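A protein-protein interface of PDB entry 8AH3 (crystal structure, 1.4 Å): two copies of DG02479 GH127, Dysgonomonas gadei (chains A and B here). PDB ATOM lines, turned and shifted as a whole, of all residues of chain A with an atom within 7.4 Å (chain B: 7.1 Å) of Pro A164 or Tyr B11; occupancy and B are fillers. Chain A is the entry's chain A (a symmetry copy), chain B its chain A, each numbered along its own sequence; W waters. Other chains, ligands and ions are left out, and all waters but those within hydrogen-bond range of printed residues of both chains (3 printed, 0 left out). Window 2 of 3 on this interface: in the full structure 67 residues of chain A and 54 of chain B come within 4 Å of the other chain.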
ATOM      1  N   GLY A  19     -10.390 -22.089  -4.707  1.00  0.00           N
ATOM      2  CA  GLY A  19     -10.690 -20.666  -4.539  1.00  0.00           C
ATOM      3  C   GLY A  19     -10.859 -19.865  -5.837  1.00  0.00           C
ATOM      4  O   GLY A  19     -11.169 -18.669  -5.774  1.00  0.00           O
ATOM      5  N   MET A  20     -10.509 -20.455  -6.996  1.00  0.00           N
ATOM      6  CA  MET A  20     -10.417 -19.745  -8.267  1.00  0.00           C
ATOM      7  C   MET A  20     -11.356 -20.441  -9.251  1.00  0.00           C
ATOM      8  O   MET A  20     -11.346 -21.676  -9.367  1.00  0.00           O
ATOM      9  CB  MET A  20      -8.991 -19.765  -8.862  1.00  0.00           C
ATOM     10  CG  MET A  20      -7.935 -18.987  -8.048  1.00  0.00           C
ATOM     11  SD  MET A  20      -8.227 -17.213  -7.949  1.00  0.00           S
ATOM     12  CE  MET A  20      -7.367 -16.758  -6.443  1.00  0.00           C
ATOM     13  N   SER A  55     -13.804  -9.332  -7.678  1.00  0.00           N
ATOM     14  CA  SER A  55     -12.422  -9.719  -7.445  1.00  0.00           C
ATOM     15  C   SER A  55     -12.040 -10.814  -8.437  1.00  0.00           C
ATOM     16  O   SER A  55     -12.815 -11.718  -8.742  1.00  0.00           O
ATOM     17  CB  SER A  55     -12.221 -10.220  -6.036  1.00  0.00           C
ATOM     18  OG  SER A  55     -12.555  -9.236  -5.079  1.00  0.00           O
ATOM     19  N   GLY A  56     -10.811 -10.707  -8.961  1.00  0.00           N
ATOM     20  CA  GLY A  56     -10.362 -11.712  -9.887  1.00  0.00           C
ATOM     21  C   GLY A  56      -8.905 -11.431 -10.259  1.00  0.00           C
ATOM     22  O   GLY A  56      -8.267 -10.503  -9.756  1.00  0.00           O
ATOM     23  N   ILE A  57      -8.406 -12.259 -11.182  1.00  0.00           N
ATOM     24  CA  ILE A  57      -7.040 -12.139 -11.669  1.00  0.00           C
ATOM     25  C   ILE A  57      -7.060 -12.475 -13.147  1.00  0.00           C
ATOM     26  O   ILE A  57      -7.286 -13.622 -13.480  1.00  0.00           O
ATOM     27  CB  ILE A  57      -6.075 -13.084 -10.946  1.00  0.00           C
ATOM     28  CG1 ILE A  57      -6.157 -12.976  -9.430  1.00  0.00           C
ATOM     29  CG2 ILE A  57      -4.664 -12.831 -11.451  1.00  0.00           C
ATOM     30  CD1 ILE A  57      -5.508 -14.099  -8.714  1.00  0.00           C
ATOM     31  N   TYR A 127       0.738 -13.003 -20.866  1.00  0.00           N
ATOM     32  CA  TYR A 127       0.600 -13.898 -19.722  1.00  0.00           C
ATOM     33  C   TYR A 127       0.899 -13.204 -18.381  1.00  0.00           C
ATOM     34  O   TYR A 127       0.967 -13.869 -17.343  1.00  0.00           O
ATOM     35  CB  TYR A 127       1.531 -15.106 -19.871  1.00  0.00           C
ATOM     36  CG  TYR A 127       1.020 -16.165 -20.828  1.00  0.00           C
ATOM     37  CD1 TYR A 127      -0.078 -16.945 -20.509  1.00  0.00           C
ATOM     38  CD2 TYR A 127       1.592 -16.276 -22.083  1.00  0.00           C
ATOM     39  CE1 TYR A 127      -0.575 -17.902 -21.392  1.00  0.00           C
ATOM     40  CE2 TYR A 127       1.139 -17.251 -22.969  1.00  0.00           C
ATOM     41  CZ  TYR A 127       0.039 -18.035 -22.630  1.00  0.00           C
ATOM     42  OH  TYR A 127      -0.421 -19.032 -23.475  1.00  0.00           O
ATOM     43  N   PHE A 128       0.986 -11.867 -18.329  1.00  0.00           N
ATOM     44  CA  PHE A 128       1.074 -11.189 -17.053  1.00  0.00           C
ATOM     45  C   PHE A 128      -0.203 -11.412 -16.241  1.00  0.00           C
ATOM     46  O   PHE A 128      -1.303 -11.323 -16.780  1.00  0.00           O
ATOM     47  CB  PHE A 128       1.309  -9.698 -17.250  1.00  0.00           C
ATOM     48  CG  PHE A 128       2.748  -9.339 -17.570  1.00  0.00           C
ATOM     49  CD1 PHE A 128       3.740  -9.533 -16.665  1.00  0.00           C
ATOM     50  CD2 PHE A 128       3.045  -8.690 -18.757  1.00  0.00           C
ATOM     51  CE1 PHE A 128       5.056  -9.198 -16.962  1.00  0.00           C
ATOM     52  CE2 PHE A 128       4.345  -8.265 -18.997  1.00  0.00           C
ATOM     53  CZ  PHE A 128       5.335  -8.557 -18.125  1.00  0.00           C
ATOM     54  N   SER A 129      -0.010 -11.705 -14.961  1.00  0.00           N
ATOM     55  CA  SER A 129      -1.110 -11.817 -14.020  1.00  0.00           C
ATOM     56  C   SER A 129      -1.548 -10.410 -13.578  1.00  0.00           C
ATOM     57  O   SER A 129      -0.747  -9.560 -13.224  1.00  0.00           O
ATOM     58  CB  SER A 129      -0.617 -12.669 -12.854  1.00  0.00           C
ATOM     59  OG  SER A 129      -1.504 -12.632 -11.745  1.00  0.00           O
ATOM     60  N   MET A 130      -2.861 -10.146 -13.624  1.00  0.00           N
ATOM     61  CA  MET A 130      -3.344  -8.812 -13.319  1.00  0.00           C
ATOM     62  C   MET A 130      -4.484  -8.905 -12.303  1.00  0.00           C
ATOM     63  O   MET A 130      -5.657  -9.106 -12.687  1.00  0.00           O
ATOM     64  CB  MET A 130      -3.822  -8.083 -14.564  1.00  0.00           C
ATOM     65  CG  MET A 130      -2.838  -8.174 -15.729  1.00  0.00           C
ATOM     66  SD  MET A 130      -3.396  -7.156 -17.095  1.00  0.00           S
ATOM     67  CE  MET A 130      -2.133  -7.543 -18.324  1.00  0.00           C
ATOM     68  N   PRO A 131      -4.129  -8.861 -11.006  1.00  0.00           N
ATOM     69  CA  PRO A 131      -5.140  -8.970  -9.925  1.00  0.00           C
ATOM     70  C   PRO A 131      -5.981  -7.706  -9.841  1.00  0.00           C
ATOM     71  O   PRO A 131      -5.524  -6.606 -10.110  1.00  0.00           O
ATOM     72  CB  PRO A 131      -4.350  -9.176  -8.635  1.00  0.00           C
ATOM     73  CG  PRO A 131      -2.947  -9.594  -9.112  1.00  0.00           C
ATOM     74  CD  PRO A 131      -2.776  -8.835 -10.430  1.00  0.00           C
ATOM     75  N   TYR A 158      -9.437 -15.517 -13.532  1.00  0.00           N
ATOM     76  CA  TYR A 158      -9.939 -16.279 -12.412  1.00  0.00           C
ATOM     77  C   TYR A 158     -10.831 -15.356 -11.579  1.00  0.00           C
ATOM     78  O   TYR A 158     -10.384 -14.297 -11.177  1.00  0.00           O
ATOM     79  CB  TYR A 158      -8.816 -16.843 -11.538  1.00  0.00           C
ATOM     80  CG  TYR A 158      -7.870 -17.793 -12.234  1.00  0.00           C
ATOM     81  CD1 TYR A 158      -8.327 -18.973 -12.783  1.00  0.00           C
ATOM     82  CD2 TYR A 158      -6.518 -17.489 -12.346  1.00  0.00           C
ATOM     83  CE1 TYR A 158      -7.484 -19.835 -13.453  1.00  0.00           C
ATOM     84  CE2 TYR A 158      -5.651 -18.357 -13.009  1.00  0.00           C
ATOM     85  CZ  TYR A 158      -6.145 -19.524 -13.551  1.00  0.00           C
ATOM     86  OH  TYR A 158      -5.319 -20.413 -14.205  1.00  0.00           O
ATOM     87  N   THR A 160     -12.680 -14.846  -7.944  1.00  0.00           N
ATOM     88  CA  THR A 160     -12.510 -15.313  -6.588  1.00  0.00           C
ATOM     89  C   THR A 160     -13.446 -14.541  -5.663  1.00  0.00           C
ATOM     90  O   THR A 160     -13.773 -13.384  -5.958  1.00  0.00           O
ATOM     91  CB  THR A 160     -11.039 -15.216  -6.166  1.00  0.00           C
ATOM     92  OG1 THR A 160     -10.872 -15.911  -4.927  1.00  0.00           O
ATOM     93  CG2 THR A 160     -10.516 -13.802  -6.053  1.00  0.00           C
ATOM     94  N   LYS A 162     -12.625 -13.647  -2.608  1.00  0.00           N
ATOM     95  CA  LYS A 162     -11.797 -12.743  -1.841  1.00  0.00           C
ATOM     96  C   LYS A 162     -10.388 -12.798  -2.418  1.00  0.00           C
ATOM     97  O   LYS A 162      -9.768 -13.857  -2.426  1.00  0.00           O
ATOM     98  CB  LYS A 162     -11.737 -13.179  -0.372  1.00  0.00           C
ATOM     99  CG  LYS A 162     -11.037 -12.193   0.557  1.00  0.00           C
ATOM    100  CD  LYS A 162     -11.104 -12.626   2.015  1.00  0.00           C
ATOM    101  CE  LYS A 162     -10.009 -12.024   2.881  1.00  0.00           C
ATOM    102  NZ  LYS A 162      -9.809 -10.585   2.575  1.00  0.00           N
ATOM    103  N   LEU A 163      -9.907 -11.646  -2.844  1.00  0.00           N
ATOM    104  CA  LEU A 163      -8.563 -11.565  -3.413  1.00  0.00           C
ATOM    105  C   LEU A 163      -7.544 -11.865  -2.337  1.00  0.00           C
ATOM    106  O   LEU A 163      -7.603 -11.245  -1.279  1.00  0.00           O
ATOM    107  CB  LEU A 163      -8.349 -10.178  -4.025  1.00  0.00           C
ATOM    108  CG  LEU A 163      -7.204 -10.088  -5.018  1.00  0.00           C
ATOM    109  CD1 LEU A 163      -7.511 -10.925  -6.258  1.00  0.00           C
ATOM    110  CD2 LEU A 163      -6.897  -8.664  -5.378  1.00  0.00           C
ATOM    111  N   PRO A 164      -6.545 -12.752  -2.564  1.00  0.00           N
ATOM    112  CA  PRO A 164      -5.411 -12.896  -1.656  1.00  0.00           C
ATOM    113  C   PRO A 164      -4.839 -11.530  -1.320  1.00  0.00           C
ATOM    114  O   PRO A 164      -4.668 -10.650  -2.195  1.00  0.00           O
ATOM    115  CB  PRO A 164      -4.441 -13.797  -2.422  1.00  0.00           C
ATOM    116  CG  PRO A 164      -5.355 -14.658  -3.242  1.00  0.00           C
ATOM    117  CD  PRO A 164      -6.507 -13.760  -3.640  1.00  0.00           C
ATOM    118  N   THR A 165      -4.558 -11.314  -0.027  1.00  0.00           N
ATOM    119  CA  THR A 165      -4.304  -9.967   0.454  1.00  0.00           C
ATOM    120  C   THR A 165      -2.896  -9.469   0.103  1.00  0.00           C
ATOM    121  O   THR A 165      -2.599  -8.296   0.264  1.00  0.00           O
ATOM    122  CB  THR A 165      -4.527  -9.867   1.988  1.00  0.00           C
ATOM    123  OG1 THR A 165      -3.665 -10.811   2.603  1.00  0.00           O
ATOM    124  CG2 THR A 165      -5.941 -10.241   2.407  1.00  0.00           C
ATOM    125  N   ASP A 166      -2.044 -10.330  -0.417  1.00  0.00           N
ATOM    126  CA  ASP A 166      -0.696  -9.929  -0.747  1.00  0.00           C
ATOM    127  C   ASP A 166      -0.576  -9.542  -2.226  1.00  0.00           C
ATOM    128  O   ASP A 166       0.500  -9.144  -2.629  1.00  0.00           O
ATOM    129  CB  ASP A 166       0.336 -11.000  -0.380  1.00  0.00           C
ATOM    130  CG  ASP A 166       0.131 -12.366  -1.004  1.00  0.00           C
ATOM    131  OD1 ASP A 166      -0.964 -12.605  -1.570  1.00  0.00           O
ATOM    132  OD2 ASP A 166       1.109 -13.193  -0.950  1.00  0.00           O
ATOM    133  N   LEU A 167      -1.658  -9.606  -3.004  1.00  0.00           N
ATOM    134  CA  LEU A 167      -1.540  -9.338  -4.444  1.00  0.00           C
ATOM    135  C   LEU A 167      -1.524  -7.841  -4.717  1.00  0.00           C
ATOM    136  O   LEU A 167      -2.297  -7.091  -4.130  1.00  0.00           O
ATOM    137  CB  LEU A 167      -2.686  -9.989  -5.212  1.00  0.00           C
ATOM    138  CG  LEU A 167      -2.636 -11.514  -5.211  1.00  0.00           C
ATOM    139  CD1 LEU A 167      -3.791 -12.045  -6.005  1.00  0.00           C
ATOM    140  CD2 LEU A 167      -1.323 -12.009  -5.792  1.00  0.00           C
ATOM    141  N   GLY A 168      -0.656  -7.439  -5.656  1.00  0.00           N
ATOM    142  CA  GLY A 168      -0.640  -6.094  -6.161  1.00  0.00           C
ATOM    143  C   GLY A 168      -1.477  -5.912  -7.417  1.00  0.00           C
ATOM    144  O   GLY A 168      -2.459  -6.607  -7.675  1.00  0.00           O
ATOM    145  N   ARG A 169      -1.096  -4.878  -8.176  1.00  0.00           N
ATOM    146  CA  ARG A 169      -1.846  -4.415  -9.332  1.00  0.00           C
ATOM    147  C   ARG A 169      -0.858  -4.119 -10.467  1.00  0.00           C
ATOM    148  O   ARG A 169       0.170  -3.485 -10.230  1.00  0.00           O
ATOM    149  CB  ARG A 169      -2.635  -3.138  -9.043  1.00  0.00           C
ATOM    150  CG  ARG A 169      -3.683  -3.293  -7.933  1.00  0.00           C
ATOM    151  CD  ARG A 169      -4.827  -4.217  -8.305  1.00  0.00           C
ATOM    152  NE  ARG A 169      -5.818  -4.271  -7.210  1.00  0.00           N
ATOM    153  CZ  ARG A 169      -5.703  -5.013  -6.113  1.00  0.00           C
ATOM    154  NH1 ARG A 169      -4.763  -5.932  -6.000  1.00  0.00           N
ATOM    155  NH2 ARG A 169      -6.549  -4.800  -5.106  1.00  0.00           N
ATOM    156  N   TYR A 327       4.447  -3.781 -11.100  1.00  0.00           N
ATOM    157  CA  TYR A 327       3.366  -3.951 -10.137  1.00  0.00           C
ATOM    158  C   TYR A 327       3.485  -2.911  -9.019  1.00  0.00           C
ATOM    159  O   TYR A 327       4.575  -2.528  -8.646  1.00  0.00           O
ATOM    160  CB  TYR A 327       3.418  -5.352  -9.509  1.00  0.00           C
ATOM    161  CG  TYR A 327       2.992  -6.419 -10.483  1.00  0.00           C
ATOM    162  CD1 TYR A 327       1.681  -6.767 -10.652  1.00  0.00           C
ATOM    163  CD2 TYR A 327       3.926  -7.023 -11.343  1.00  0.00           C
ATOM    164  CE1 TYR A 327       1.274  -7.687 -11.616  1.00  0.00           C
ATOM    165  CE2 TYR A 327       3.525  -7.931 -12.299  1.00  0.00           C
ATOM    166  CZ  TYR A 327       2.202  -8.253 -12.479  1.00  0.00           C
ATOM    167  OH  TYR A 327       1.787  -9.152 -13.402  1.00  0.00           O
ATOM    168  N   GLN B   3      -0.206 -21.202   0.646  1.00  0.00           N
ATOM    169  CA  GLN B   3       0.060 -21.812  -0.683  1.00  0.00           C
ATOM    170  C   GLN B   3      -0.661 -20.976  -1.748  1.00  0.00           C
ATOM    171  O   GLN B   3      -1.814 -20.508  -1.608  1.00  0.00           O
ATOM    172  CB  GLN B   3      -0.357 -23.283  -0.718  1.00  0.00           C
ATOM    173  CG  GLN B   3       0.247 -24.073  -1.879  1.00  0.00           C
ATOM    174  CD  GLN B   3       1.707 -24.430  -1.703  1.00  0.00           C
ATOM    175  OE1 GLN B   3       2.522 -24.308  -2.616  1.00  0.00           O
ATOM    176  NE2 GLN B   3       2.043 -24.946  -0.534  1.00  0.00           N
ATOM    177  N   ASN B   4      -0.003 -20.849  -2.890  1.00  0.00           N
ATOM    178  CA  ASN B   4      -0.581 -19.978  -3.909  1.00  0.00           C
ATOM    179  C   ASN B   4      -1.750 -20.692  -4.572  1.00  0.00           C
ATOM    180  O   ASN B   4      -1.700 -21.897  -4.842  1.00  0.00           O
ATOM    181  CB  ASN B   4       0.443 -19.561  -4.949  1.00  0.00           C
ATOM    182  CG  ASN B   4       1.584 -18.705  -4.413  1.00  0.00           C
ATOM    183  OD1 ASN B   4       1.521 -18.139  -3.328  1.00  0.00           O
ATOM    184  ND2 ASN B   4       2.617 -18.567  -5.218  1.00  0.00           N
ATOM    185  N   PRO B   5      -2.814 -19.954  -4.949  1.00  0.00           N
ATOM    186  CA  PRO B   5      -3.959 -20.614  -5.598  1.00  0.00           C
ATOM    187  C   PRO B   5      -3.748 -20.854  -7.085  1.00  0.00           C
ATOM    188  O   PRO B   5      -4.623 -21.435  -7.726  1.00  0.00           O
ATOM    189  CB  PRO B   5      -5.112 -19.617  -5.389  1.00  0.00           C
ATOM    190  CG  PRO B   5      -4.374 -18.284  -5.278  1.00  0.00           C
ATOM    191  CD  PRO B   5      -3.111 -18.592  -4.498  1.00  0.00           C
ATOM    192  N   VAL B   6      -2.673 -20.275  -7.665  1.00  0.00           N
ATOM    193  CA  VAL B   6      -2.390 -20.417  -9.082  1.00  0.00           C
ATOM    194  C   VAL B   6      -0.923 -20.844  -9.136  1.00  0.00           C
ATOM    195  O   VAL B   6      -0.117 -20.244  -8.429  1.00  0.00           O
ATOM    196  CB  VAL B   6      -2.618 -19.111  -9.872  1.00  0.00           C
ATOM    197  CG1 VAL B   6      -2.260 -19.256 -11.345  1.00  0.00           C
ATOM    198  CG2 VAL B   6      -4.038 -18.575  -9.735  1.00  0.00           C
ATOM    199  N   PRO B   7      -0.537 -21.855  -9.946  1.00  0.00           N
ATOM    200  CA  PRO B   7       0.794 -22.437  -9.852  1.00  0.00           C
ATOM    201  C   PRO B   7       2.039 -21.772 -10.424  1.00  0.00           C
ATOM    202  O   PRO B   7       3.129 -22.184 -10.087  1.00  0.00           O
ATOM    203  CB  PRO B   7       0.630 -23.788 -10.559  1.00  0.00           C
ATOM    204  CG  PRO B   7      -0.478 -23.568 -11.562  1.00  0.00           C
ATOM    205  CD  PRO B   7      -1.423 -22.645 -10.817  1.00  0.00           C
ATOM    206  N   GLY B   8       1.926 -20.800 -11.276  1.00  0.00           N
ATOM    207  CA  GLY B   8       3.165 -20.409 -11.969  1.00  0.00           C
ATOM    208  C   GLY B   8       3.923 -19.201 -11.391  1.00  0.00           C
ATOM    209  O   GLY B   8       3.511 -18.522 -10.431  1.00  0.00           O
ATOM    210  N   THR B   9       4.990 -18.822 -12.107  1.00  0.00           N
ATOM    211  CA  THR B   9       5.744 -17.652 -11.740  1.00  0.00           C
ATOM    212  C   THR B   9       4.952 -16.368 -12.010  1.00  0.00           C
ATOM    213  O   THR B   9       5.144 -15.389 -11.312  1.00  0.00           O
ATOM    214  CB  THR B   9       7.068 -17.606 -12.514  1.00  0.00           C
ATOM    215  OG1 THR B   9       7.851 -18.701 -12.047  1.00  0.00           O
ATOM    216  CG2 THR B   9       7.852 -16.351 -12.260  1.00  0.00           C
ATOM    217  N   MET B  10       4.119 -16.349 -13.044  1.00  0.00           N
ATOM    218  CA  MET B  10       3.435 -15.091 -13.346  1.00  0.00           C
ATOM    219  C   MET B  10       2.500 -14.691 -12.198  1.00  0.00           C
ATOM    220  O   MET B  10       2.443 -13.524 -11.807  1.00  0.00           O
ATOM    221  CB  MET B  10       2.708 -15.137 -14.690  1.00  0.00           C
ATOM    222  CG  MET B  10       3.638 -15.395 -15.863  1.00  0.00           C
ATOM    223  SD  MET B  10       5.201 -14.455 -15.931  1.00  0.00           S
ATOM    224  CE  MET B  10       4.544 -12.833 -16.289  1.00  0.00           C
ATOM    225  N   TYR B  11       1.816 -15.654 -11.584  1.00  0.00           N
ATOM    226  CA  TYR B  11       1.013 -15.329 -10.420  1.00  0.00           C
ATOM    227  C   TYR B  11       1.904 -14.756  -9.306  1.00  0.00           C
ATOM    228  O   TYR B  11       1.587 -13.739  -8.702  1.00  0.00           O
ATOM    229  CB  TYR B  11       0.260 -16.550  -9.887  1.00  0.00           C
ATOM    230  CG  TYR B  11      -0.454 -16.277  -8.590  1.00  0.00           C
ATOM    231  CD1 TYR B  11      -1.727 -15.730  -8.621  1.00  0.00           C
ATOM    232  CD2 TYR B  11       0.099 -16.528  -7.358  1.00  0.00           C
ATOM    233  CE1 TYR B  11      -2.437 -15.453  -7.460  1.00  0.00           C
ATOM    234  CE2 TYR B  11      -0.570 -16.218  -6.165  1.00  0.00           C
ATOM    235  CZ  TYR B  11      -1.860 -15.696  -6.223  1.00  0.00           C
ATOM    236  OH  TYR B  11      -2.510 -15.368  -5.051  1.00  0.00           O
ATOM    237  N   GLU B  12       3.019 -15.433  -9.026  1.00  0.00           N
ATOM    238  CA  GLU B  12       3.928 -15.042  -7.952  1.00  0.00           C
ATOM    239  C   GLU B  12       4.459 -13.633  -8.186  1.00  0.00           C
ATOM    240  O   GLU B  12       4.690 -12.867  -7.242  1.00  0.00           O
ATOM    241  CB  GLU B  12       5.114 -16.021  -7.799  1.00  0.00           C
ATOM    242  CG  GLU B  12       4.762 -17.415  -7.329  1.00  0.00           C
ATOM    243  CD  GLU B  12       5.695 -18.608  -7.642  1.00  0.00           C
ATOM    244  OE1 GLU B  12       6.836 -18.365  -8.165  1.00  0.00           O
ATOM    245  OE2 GLU B  12       5.286 -19.869  -7.402  1.00  0.00           O
ATOM    246  N   LEU B  13       4.706 -13.278  -9.443  1.00  0.00           N
ATOM    247  CA  LEU B  13       5.260 -11.988  -9.792  1.00  0.00           C
ATOM    248  C   LEU B  13       4.259 -10.880  -9.462  1.00  0.00           C
ATOM    249  O   LEU B  13       4.632  -9.710  -9.315  1.00  0.00           O
ATOM    250  CB  LEU B  13       5.599 -12.009 -11.279  1.00  0.00           C
ATOM    251  CG  LEU B  13       6.386 -10.849 -11.825  1.00  0.00           C
ATOM    252  CD1 LEU B  13       7.814 -10.759 -11.225  1.00  0.00           C
ATOM    253  CD2 LEU B  13       6.508 -10.981 -13.331  1.00  0.00           C
ATOM    254  N   SER B  14       2.957 -11.212  -9.339  1.00  0.00           N
ATOM    255  CA  SER B  14       1.974 -10.179  -9.012  1.00  0.00           C
ATOM    256  C   SER B  14       1.770 -10.025  -7.504  1.00  0.00           C
ATOM    257  O   SER B  14       0.971  -9.206  -7.080  1.00  0.00           O
ATOM    258  CB  SER B  14       0.650 -10.455  -9.692  1.00  0.00           C
ATOM    259  OG  SER B  14       0.005 -11.653  -9.207  1.00  0.00           O
ATOM    260  N   GLN B  15       2.535 -10.740  -6.703  1.00  0.00           N
ATOM    261  CA  GLN B  15       2.490 -10.677  -5.236  1.00  0.00           C
ATOM    262  C   GLN B  15       3.457  -9.613  -4.745  1.00  0.00           C
ATOM    263  O   GLN B  15       4.599  -9.516  -5.243  1.00  0.00           O
ATOM    264  CB  GLN B  15       2.927 -11.986  -4.567  1.00  0.00           C
ATOM    265  CG  GLN B  15       1.962 -13.121  -4.713  1.00  0.00           C
ATOM    266  CD  GLN B  15       2.490 -14.406  -4.115  1.00  0.00           C
ATOM    267  OE1 GLN B  15       3.602 -14.837  -4.415  1.00  0.00           O
ATOM    268  NE2 GLN B  15       1.689 -15.014  -3.265  1.00  0.00           N
HETATM  269  O   HOH W   1       0.003 -15.982  -0.600  1.00  0.00           O
HETATM  270  O   HOH W   2       2.701 -11.741 -13.847  1.00  0.00           O
HETATM  271  O   HOH W   3      -1.073 -14.921  -2.865  1.00  0.00           O
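Among the printed residues, merely in contact across the chains: Met A20 with Pro B5, Ile A57 with Tyr B11, Tyr A127 with Met B10, Phe A128 with Met B10, Ser A129 with Met B10, Ser A129 with Tyr B11, Pro A131 with Ser B14, Tyr A158 with Val B6, Pro A164 with Tyr B11, Leu A167 with Tyr B11, Leu A167 with Ser B14, Leu A167 with Gln B15, Tyr A327 with Leu B13 and Tyr A327 with Ser B14.
Thr A160 touches none of the printed residues of chain B.
Printed residues of chain B within 4 Å of Pro A164: Tyr B11.
Of the printed residues of chain B, Leu A167 touches Tyr B11 (3.6 Å), Ser B14 (3.6 Å) and Gln B15 (3.6 Å).
Tyr B11 touches just these residues of chain A: Ile A57 (3.6 Å), Ser A129 (3.9 Å), Pro A164 (3.4 Å) and Leu A167 (3.6 Å).
Of the printed residues of chain A, Gln B15 touches Asp A166 (3.0 Å) and Leu A167 (3.6 Å).
The nearest residue of chain B that does not touch Pro A164 is Pro B5 (4.3 Å).
The nearest residue of chain A that does not touch Tyr B11 is Asp A166 (4.7 Å).
No position is printed for both chains.
Of the 17 pairs that touch across the chains among the printed residues, none has its exchanged pair printed and touching as well.
N of Gly A168 sits at hydrogen-bond distance from O of Ser B14 (2.8 Å).
NE2 of Gln B15 is in hydrogen-bond range of OD2 of Asp A166 (3.0 Å).
The side-chain hydroxyl (OG) of Ser B14 lies within hydrogen-bond range of the side-chain hydroxyl (OG) of Ser A129 (3.1 Å).
NE2 of Gln B15 is in hydrogen-bond range of OD1 of Asn B4.
O of Ser A129 is in hydrogen-bond range of OH of Tyr A327 (2.6 Å).
O of Tyr B11 lies within hydrogen-bond range of OG of Ser B14 (2.7 Å).
N of Ile A57 sits at hydrogen-bond distance from O of Tyr A158, at 2.8 Å.
The backbone carbonyl oxygen (O) of Leu A167 lies within hydrogen-bond range of the guanidinium group (NH1) of Arg A169 (3.3 Å).
Water W3 lies within hydrogen-bond range of the side-chain hydroxyl of Tyr B11 (2.7 Å), the side-chain carboxylate of Asp A166 (2.7 Å) and the side-chain amide nitrogen of Gln B15 (2.8 Å).
Water W2 lies within hydrogen-bond range of O of Met B10 (2.7 Å), OH of Tyr A327 (2.8 Å) and N of Ser A129 (2.9 Å).
Water W1 lies within hydrogen-bond range of OD2 of Asp A166 and NE2 of Gln B15.
Of the 21 printed residues of chain A, 12 touch a printed residue of chain B.
Printed residues of chain A that touch a printed residue of chain B: Met A20, Ile A57, Tyr A127, Phe A128, Ser A129, Pro A131, Tyr A158, Pro A164, Asp A166, Leu A167, Gly A168 and Tyr A327.
Hydrophobic or aromatic side chains of chain A that line the printed part of chain B: Met A20, Ile A57, Phe A128, Pro A131, Tyr A158, Pro A164, Leu A167 and Tyr A327.
Printed residues of chain B that touch a printed residue of chain A: Pro B5, Val B6, Met B10, Tyr B11, Leu B13, Ser B14 and Gln B15.
Hydrophobic or aromatic side chains of chain B that line the printed part of chain A: Pro B5, Val B6, Met B10 and Tyr B11.
Among the printed residues, 17 pairs touch across the chains.
Among the printed residues, no Asp or Glu carboxylate lies within 4 Å of a Lys or Arg side-chain nitrogen of the other chain.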
